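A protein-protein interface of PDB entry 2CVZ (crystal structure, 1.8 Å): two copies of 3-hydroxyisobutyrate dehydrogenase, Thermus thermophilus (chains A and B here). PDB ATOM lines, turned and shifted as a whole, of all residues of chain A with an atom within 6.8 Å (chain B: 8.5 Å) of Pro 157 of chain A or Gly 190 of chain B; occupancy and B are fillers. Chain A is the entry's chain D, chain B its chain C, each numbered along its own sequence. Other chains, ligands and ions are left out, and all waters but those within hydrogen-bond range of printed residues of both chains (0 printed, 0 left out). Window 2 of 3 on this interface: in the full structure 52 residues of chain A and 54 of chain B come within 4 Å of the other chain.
Printed residues of chain B within 4 Å of Arg 98 of chain A: Gln 189 (2.8 Å).
Printed residues of chain B within 4 Å of His 154 of chain A: Lys 195.
Printed residues of chain B within 4 Å of Val 155 of chain A: Val 191, Ser 192 and Lys 195.
No residue of chain B comes within 4 Å of Gly 156 of chain A.
Of chain B, only Gly 190 comes within 4 Å of Pro 157 of chain A.
Printed residues of chain A within 4 Å of Gly 190 of chain B: Pro 157 (3.4 Å).
Printed residues of chain A within 4 Å of Val 191 of chain B: Val 155 (3.5 Å) and Ala 160 (3.6 Å).
Printed residues of chain A within 4 Å of Lys 195 of chain B: His 154 and Val 155.
The nearest residue of chain B that does not touch Pro 157 of chain A is Val 191 of chain B (4.9 Å).
The nearest residue of chain A that does not touch Gly 190 of chain B is Gly 156 of chain A (4.2 Å).
No position is printed for both chains.
Of the 7 pairs that touch across the chains among the printed residues, none has its exchanged pair printed and touching as well.
The backbone NH (N) of Ser 192 of chain B is in hydrogen-bond range of the backbone carbonyl oxygen (O) of Val 155 of chain A (2.9 Å).
The side-chain amide oxygen (OE1) of Gln 189 of chain B sits at hydrogen-bond distance from the guanidinium group (NH2) of Arg 98 of chain A (2.8 Å).
Hydrophobic or aromatic side chains of chain A that line the printed part of chain B: Val 155, Pro 157 and Ala 160.
Along chain A the printed residues that touch a printed residue of chain B span positions 98 to 160.
Hydrophobic or aromatic side chains of chain B that line the printed part of chain A: Val 191.
Among the printed residues, 7 pairs touch across the chains.
The backbone NH (N) of Val 191 of chain B lies within hydrogen-bond range of the backbone carbonyl oxygen (O) of Leu 186 of chain B, at 3.1 Å.
The backbone carbonyl oxygen (O) of Leu 132 of chain A lies within hydrogen-bond range of the backbone NH (N) of Val 155 of chain A (2.9 Å).
OG of Ser 192 of chain B sits at hydrogen-bond distance from N of Lys 195 of chain B, at 3.2 Å.
The backbone carbonyl oxygen of Gly 134 of chain A is in hydrogen-bond range of a ring nitrogen (NE2) of His 154 of chain A, at 2.7 Å.
The side-chain carboxylate (OD1) of Asp 113 of chain A sits at hydrogen-bond distance from the backbone NH (N) of Ala 160 of chain A (3.3 Å).
The guanidinium group of Arg 98 of chain A sits at hydrogen-bond distance from the backbone carbonyl oxygen of Val 158 of chain A (3.0 Å).
Among the printed residues, pairs that only touch across the chains: His 154 of chain A with Lys 195 of chain B (3.4 Å), Val 155 of chain A with Val 191 of chain B (3.5 Å), Val 155 of chain A with Lys 195 of chain B (3.96 Å), Pro 157 of chain A with Gly 190 of chain B (3.4 Å) and Ala 160 of chain A with Val 191 of chain B (3.6 Å).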
ATOM      1  N   ARG A  98      18.046   3.617 -17.400  1.00  0.00           N
ATOM      2  CA  ARG A  98      17.167   4.762 -17.193  1.00  0.00           C
ATOM      3  C   ARG A  98      18.027   6.025 -17.180  1.00  0.00           C
ATOM      4  O   ARG A  98      17.638   7.060 -17.725  1.00  0.00           O
ATOM      5  CB  ARG A  98      16.395   4.627 -15.876  1.00  0.00           C
ATOM      6  CG  ARG A  98      15.466   3.426 -15.849  1.00  0.00           C
ATOM      7  CD  ARG A  98      14.578   3.396 -14.614  1.00  0.00           C
ATOM      8  NE  ARG A  98      13.679   2.243 -14.645  1.00  0.00           N
ATOM      9  CZ  ARG A  98      13.923   1.074 -14.060  1.00  0.00           C
ATOM     10  NH1 ARG A  98      15.046   0.886 -13.380  1.00  0.00           N
ATOM     11  NH2 ARG A  98      13.044   0.084 -14.163  1.00  0.00           N
ATOM     12  N   ASP A 113      14.371   0.357 -24.123  1.00  0.00           N
ATOM     13  CA  ASP A 113      15.064  -0.902 -23.905  1.00  0.00           C
ATOM     14  C   ASP A 113      14.218  -1.974 -24.575  1.00  0.00           C
ATOM     15  O   ASP A 113      12.998  -2.019 -24.394  1.00  0.00           O
ATOM     16  CB  ASP A 113      15.294  -1.200 -22.410  1.00  0.00           C
ATOM     17  CG  ASP A 113      14.080  -0.923 -21.538  1.00  0.00           C
ATOM     18  OD1 ASP A 113      13.787  -1.773 -20.668  1.00  0.00           O
ATOM     19  OD2 ASP A 113      13.441   0.141 -21.686  1.00  0.00           O
ATOM     20  N   LEU A 132       9.574  -4.530 -24.840  1.00  0.00           N
ATOM     21  CA  LEU A 132       9.855  -3.100 -24.906  1.00  0.00           C
ATOM     22  C   LEU A 132       9.526  -2.294 -23.664  1.00  0.00           C
ATOM     23  O   LEU A 132       8.473  -2.471 -23.051  1.00  0.00           O
ATOM     24  CB  LEU A 132       9.090  -2.477 -26.078  1.00  0.00           C
ATOM     25  CG  LEU A 132       9.496  -2.800 -27.515  1.00  0.00           C
ATOM     26  CD1 LEU A 132       8.404  -2.322 -28.467  1.00  0.00           C
ATOM     27  CD2 LEU A 132      10.815  -2.119 -27.835  1.00  0.00           C
ATOM     28  N   GLY A 133      10.438  -1.391 -23.319  1.00  0.00           N
ATOM     29  CA  GLY A 133      10.239  -0.504 -22.189  1.00  0.00           C
ATOM     30  C   GLY A 133      10.337   0.912 -22.734  1.00  0.00           C
ATOM     31  O   GLY A 133      11.271   1.224 -23.473  1.00  0.00           O
ATOM     32  N   GLY A 134       9.377   1.768 -22.401  1.00  0.00           N
ATOM     33  CA  GLY A 134       9.427   3.135 -22.896  1.00  0.00           C
ATOM     34  C   GLY A 134       8.068   3.792 -23.068  1.00  0.00           C
ATOM     35  O   GLY A 134       7.045   3.195 -22.740  1.00  0.00           O
ATOM     36  N   PRO A 135       8.030   5.037 -23.576  1.00  0.00           N
ATOM     37  CA  PRO A 135       6.794   5.798 -23.801  1.00  0.00           C
ATOM     38  C   PRO A 135       5.910   5.130 -24.851  1.00  0.00           C
ATOM     39  O   PRO A 135       6.401   4.645 -25.871  1.00  0.00           O
ATOM     40  CB  PRO A 135       7.305   7.159 -24.274  1.00  0.00           C
ATOM     41  CG  PRO A 135       8.648   7.268 -23.632  1.00  0.00           C
ATOM     42  CD  PRO A 135       9.210   5.882 -23.831  1.00  0.00           C
ATOM     43  N   HIS A 154       4.891  -4.461 -25.177  1.00  0.00           N
ATOM     44  CA  HIS A 154       5.252  -3.258 -24.428  1.00  0.00           C
ATOM     45  C   HIS A 154       4.996  -3.617 -22.963  1.00  0.00           C
ATOM     46  O   HIS A 154       3.848  -3.754 -22.547  1.00  0.00           O
ATOM     47  CB  HIS A 154       4.358  -2.082 -24.830  1.00  0.00           C
ATOM     48  CG  HIS A 154       4.716  -0.794 -24.157  1.00  0.00           C
ATOM     49  ND1 HIS A 154       3.896   0.316 -24.188  1.00  0.00           N
ATOM     50  CD2 HIS A 154       5.812  -0.432 -23.447  1.00  0.00           C
ATOM     51  CE1 HIS A 154       4.473   1.303 -23.526  1.00  0.00           C
ATOM     52  NE2 HIS A 154       5.636   0.876 -23.068  1.00  0.00           N
ATOM     53  N   VAL A 155       6.061  -3.772 -22.183  1.00  0.00           N
ATOM     54  CA  VAL A 155       5.903  -4.173 -20.789  1.00  0.00           C
ATOM     55  C   VAL A 155       5.885  -3.071 -19.733  1.00  0.00           C
ATOM     56  O   VAL A 155       5.484  -3.317 -18.596  1.00  0.00           O
ATOM     57  CB  VAL A 155       6.977  -5.220 -20.402  1.00  0.00           C
ATOM     58  CG1 VAL A 155       6.770  -6.493 -21.216  1.00  0.00           C
ATOM     59  CG2 VAL A 155       8.372  -4.660 -20.640  1.00  0.00           C
ATOM     60  N   GLY A 156       6.307  -1.865 -20.101  1.00  0.00           N
ATOM     61  CA  GLY A 156       6.310  -0.772 -19.142  1.00  0.00           C
ATOM     62  C   GLY A 156       7.216   0.379 -19.538  1.00  0.00           C
ATOM     63  O   GLY A 156       7.631   0.468 -20.693  1.00  0.00           O
ATOM     64  N   PRO A 157       7.538   1.283 -18.596  1.00  0.00           N
ATOM     65  CA  PRO A 157       8.403   2.446 -18.835  1.00  0.00           C
ATOM     66  C   PRO A 157       9.836   1.999 -19.095  1.00  0.00           C
ATOM     67  O   PRO A 157      10.157   0.822 -18.929  1.00  0.00           O
ATOM     68  CB  PRO A 157       8.296   3.238 -17.528  1.00  0.00           C
ATOM     69  CG  PRO A 157       6.994   2.775 -16.929  1.00  0.00           C
ATOM     70  CD  PRO A 157       7.017   1.304 -17.220  1.00  0.00           C
ATOM     71  N   VAL A 158      10.692   2.939 -19.491  1.00  0.00           N
ATOM     72  CA  VAL A 158      12.093   2.631 -19.756  1.00  0.00           C
ATOM     73  C   VAL A 158      12.663   1.797 -18.615  1.00  0.00           C
ATOM     74  O   VAL A 158      12.479   2.126 -17.439  1.00  0.00           O
ATOM     75  CB  VAL A 158      12.940   3.917 -19.904  1.00  0.00           C
ATOM     76  CG1 VAL A 158      14.409   3.560 -20.084  1.00  0.00           C
ATOM     77  CG2 VAL A 158      12.453   4.718 -21.094  1.00  0.00           C
ATOM     78  N   GLY A 159      13.341   0.710 -18.969  1.00  0.00           N
ATOM     79  CA  GLY A 159      13.924  -0.162 -17.968  1.00  0.00           C
ATOM     80  C   GLY A 159      13.113  -1.421 -17.721  1.00  0.00           C
ATOM     81  O   GLY A 159      13.655  -2.432 -17.269  1.00  0.00           O
ATOM     82  N   ALA A 160      11.818  -1.371 -18.024  1.00  0.00           N
ATOM     83  CA  ALA A 160      10.935  -2.516 -17.814  1.00  0.00           C
ATOM     84  C   ALA A 160      11.304  -3.710 -18.691  1.00  0.00           C
ATOM     85  O   ALA A 160      11.166  -4.863 -18.276  1.00  0.00           O
ATOM     86  CB  ALA A 160       9.483  -2.106 -18.066  1.00  0.00           C
ATOM     87  N   GLY A 161      11.762  -3.436 -19.909  1.00  0.00           N
ATOM     88  CA  GLY A 161      12.151  -4.513 -20.803  1.00  0.00           C
ATOM     89  C   GLY A 161      13.340  -5.262 -20.233  1.00  0.00           C
ATOM     90  O   GLY A 161      13.334  -6.492 -20.138  1.00  0.00           O
ATOM     91  N   LEU B 183       7.474 -11.475 -10.162  1.00  0.00           N
ATOM     92  CA  LEU B 183       6.387 -10.604 -10.598  1.00  0.00           C
ATOM     93  C   LEU B 183       6.152  -9.472  -9.607  1.00  0.00           C
ATOM     94  O   LEU B 183       5.843  -8.349 -10.000  1.00  0.00           O
ATOM     95  CB  LEU B 183       5.102 -11.415 -10.780  1.00  0.00           C
ATOM     96  CG  LEU B 183       5.119 -12.341 -11.997  1.00  0.00           C
ATOM     97  CD1 LEU B 183       3.951 -13.308 -11.953  1.00  0.00           C
ATOM     98  CD2 LEU B 183       5.075 -11.493 -13.256  1.00  0.00           C
ATOM     99  N   LEU B 184       6.300  -9.774  -8.322  1.00  0.00           N
ATOM    100  CA  LEU B 184       6.110  -8.772  -7.283  1.00  0.00           C
ATOM    101  C   LEU B 184       7.107  -7.642  -7.519  1.00  0.00           C
ATOM    102  O   LEU B 184       6.741  -6.470  -7.517  1.00  0.00           O
ATOM    103  CB  LEU B 184       6.321  -9.408  -5.904  1.00  0.00           C
ATOM    104  CG  LEU B 184       5.933  -8.628  -4.640  1.00  0.00           C
ATOM    105  CD1 LEU B 184       6.867  -7.452  -4.431  1.00  0.00           C
ATOM    106  CD2 LEU B 184       4.492  -8.164  -4.760  1.00  0.00           C
ATOM    107  N   ALA B 185       8.369  -8.003  -7.731  1.00  0.00           N
ATOM    108  CA  ALA B 185       9.416  -7.020  -7.982  1.00  0.00           C
ATOM    109  C   ALA B 185       9.113  -6.199  -9.236  1.00  0.00           C
ATOM    110  O   ALA B 185       9.261  -4.977  -9.241  1.00  0.00           O
ATOM    111  CB  ALA B 185      10.759  -7.717  -8.130  1.00  0.00           C
ATOM    112  N   LEU B 186       8.682  -6.872 -10.299  1.00  0.00           N
ATOM    113  CA  LEU B 186       8.370  -6.177 -11.547  1.00  0.00           C
ATOM    114  C   LEU B 186       7.221  -5.177 -11.395  1.00  0.00           C
ATOM    115  O   LEU B 186       7.347  -4.023 -11.803  1.00  0.00           O
ATOM    116  CB  LEU B 186       8.040  -7.188 -12.650  1.00  0.00           C
ATOM    117  CG  LEU B 186       9.217  -8.070 -13.080  1.00  0.00           C
ATOM    118  CD1 LEU B 186       8.752  -9.121 -14.076  1.00  0.00           C
ATOM    119  CD2 LEU B 186      10.310  -7.198 -13.687  1.00  0.00           C
ATOM    120  N   VAL B 187       6.109  -5.619 -10.810  1.00  0.00           N
ATOM    121  CA  VAL B 187       4.956  -4.738 -10.620  1.00  0.00           C
ATOM    122  C   VAL B 187       5.339  -3.505  -9.804  1.00  0.00           C
ATOM    123  O   VAL B 187       4.891  -2.402 -10.059  1.00  0.00           O
ATOM    124  CB  VAL B 187       3.806  -5.489  -9.927  1.00  0.00           C
ATOM    125  CG1 VAL B 187       2.684  -4.503  -9.570  1.00  0.00           C
ATOM    126  CG2 VAL B 187       3.243  -6.567 -10.838  1.00  0.00           C
ATOM    127  N   LYS B 188       6.185  -3.727  -8.783  1.00  0.00           N
ATOM    128  CA  LYS B 188       6.572  -2.605  -7.925  1.00  0.00           C
ATOM    129  C   LYS B 188       7.333  -1.507  -8.681  1.00  0.00           C
ATOM    130  O   LYS B 188       7.351  -0.347  -8.287  1.00  0.00           O
ATOM    131  CB  LYS B 188       7.401  -3.154  -6.766  1.00  0.00           C
ATOM    132  CG  LYS B 188       7.357  -2.243  -5.536  1.00  0.00           C
ATOM    133  CD  LYS B 188       5.977  -2.218  -4.879  1.00  0.00           C
ATOM    134  CE  LYS B 188       5.894  -1.213  -3.725  1.00  0.00           C
ATOM    135  NZ  LYS B 188       4.681  -1.459  -2.945  1.00  0.00           N
ATOM    136  N   GLN B 189       8.018  -1.870  -9.785  1.00  0.00           N
ATOM    137  CA  GLN B 189       8.719  -0.808 -10.514  1.00  0.00           C
ATOM    138  C   GLN B 189       7.999  -0.345 -11.783  1.00  0.00           C
ATOM    139  O   GLN B 189       8.620   0.173 -12.705  1.00  0.00           O
ATOM    140  CB  GLN B 189      10.171  -1.214 -10.826  1.00  0.00           C
ATOM    141  CG  GLN B 189      10.324  -2.576 -11.535  1.00  0.00           C
ATOM    142  CD  GLN B 189      11.794  -2.798 -11.870  1.00  0.00           C
ATOM    143  OE1 GLN B 189      12.362  -2.224 -12.779  1.00  0.00           O
ATOM    144  NE2 GLN B 189      12.414  -3.701 -11.076  1.00  0.00           N
ATOM    145  N   GLY B 190       6.686  -0.536 -11.826  1.00  0.00           N
ATOM    146  CA  GLY B 190       5.910  -0.073 -12.965  1.00  0.00           C
ATOM    147  C   GLY B 190       5.673  -1.016 -14.125  1.00  0.00           C
ATOM    148  O   GLY B 190       5.075  -0.617 -15.129  1.00  0.00           O
ATOM    149  N   VAL B 191       6.131  -2.256 -14.005  1.00  0.00           N
ATOM    150  CA  VAL B 191       5.940  -3.230 -15.072  1.00  0.00           C
ATOM    151  C   VAL B 191       4.543  -3.839 -15.025  1.00  0.00           C
ATOM    152  O   VAL B 191       4.009  -4.105 -13.950  1.00  0.00           O
ATOM    153  CB  VAL B 191       6.965  -4.379 -14.970  1.00  0.00           C
ATOM    154  CG1 VAL B 191       6.713  -5.406 -16.069  1.00  0.00           C
ATOM    155  CG2 VAL B 191       8.367  -3.827 -15.060  1.00  0.00           C
ATOM    156  N   SER B 192       3.952  -4.051 -16.198  1.00  0.00           N
ATOM    157  CA  SER B 192       2.628  -4.660 -16.289  1.00  0.00           C
ATOM    158  C   SER B 192       2.772  -6.165 -16.072  1.00  0.00           C
ATOM    159  O   SER B 192       3.496  -6.833 -16.811  1.00  0.00           O
ATOM    160  CB  SER B 192       2.017  -4.402 -17.669  1.00  0.00           C
ATOM    161  OG  SER B 192       0.898  -5.241 -17.886  1.00  0.00           O
ATOM    162  N   ALA B 193       2.092  -6.696 -15.057  1.00  0.00           N
ATOM    163  CA  ALA B 193       2.165  -8.127 -14.758  1.00  0.00           C
ATOM    164  C   ALA B 193       1.625  -8.946 -15.927  1.00  0.00           C
ATOM    165  O   ALA B 193       2.174  -9.990 -16.286  1.00  0.00           O
ATOM    166  CB  ALA B 193       1.367  -8.441 -13.495  1.00  0.00           C
ATOM    167  N   LYS B 195       1.480  -8.115 -19.175  1.00  0.00           N
ATOM    168  CA  LYS B 195       2.419  -8.073 -20.291  1.00  0.00           C
ATOM    169  C   LYS B 195       3.691  -8.851 -19.983  1.00  0.00           C
ATOM    170  O   LYS B 195       4.247  -9.518 -20.859  1.00  0.00           O
ATOM    171  CB  LYS B 195       2.759  -6.621 -20.639  1.00  0.00           C
ATOM    172  CG  LYS B 195       1.584  -5.831 -21.210  1.00  0.00           C
ATOM    173  CD  LYS B 195       1.129  -6.417 -22.540  1.00  0.00           C
ATOM    174  CE  LYS B 195       0.019  -5.588 -23.176  1.00  0.00           C
ATOM    175  NZ  LYS B 195      -1.211  -5.566 -22.341  1.00  0.00           N
ATOM    176  N   VAL B 286       1.457  -4.393  -2.649  1.00  0.00           N
ATOM    177  CA  VAL B 286       0.916  -4.202  -3.984  1.00  0.00           C
ATOM    178  C   VAL B 286       0.372  -5.529  -4.498  1.00  0.00           C
ATOM    179  O   VAL B 286       0.868  -6.595  -4.128  1.00  0.00           O
ATOM    180  CB  VAL B 286       2.006  -3.689  -4.952  1.00  0.00           C
ATOM    181  CG1 VAL B 286       3.088  -4.743  -5.121  1.00  0.00           C
ATOM    182  CG2 VAL B 286       1.393  -3.324  -6.295  1.00  0.00           C
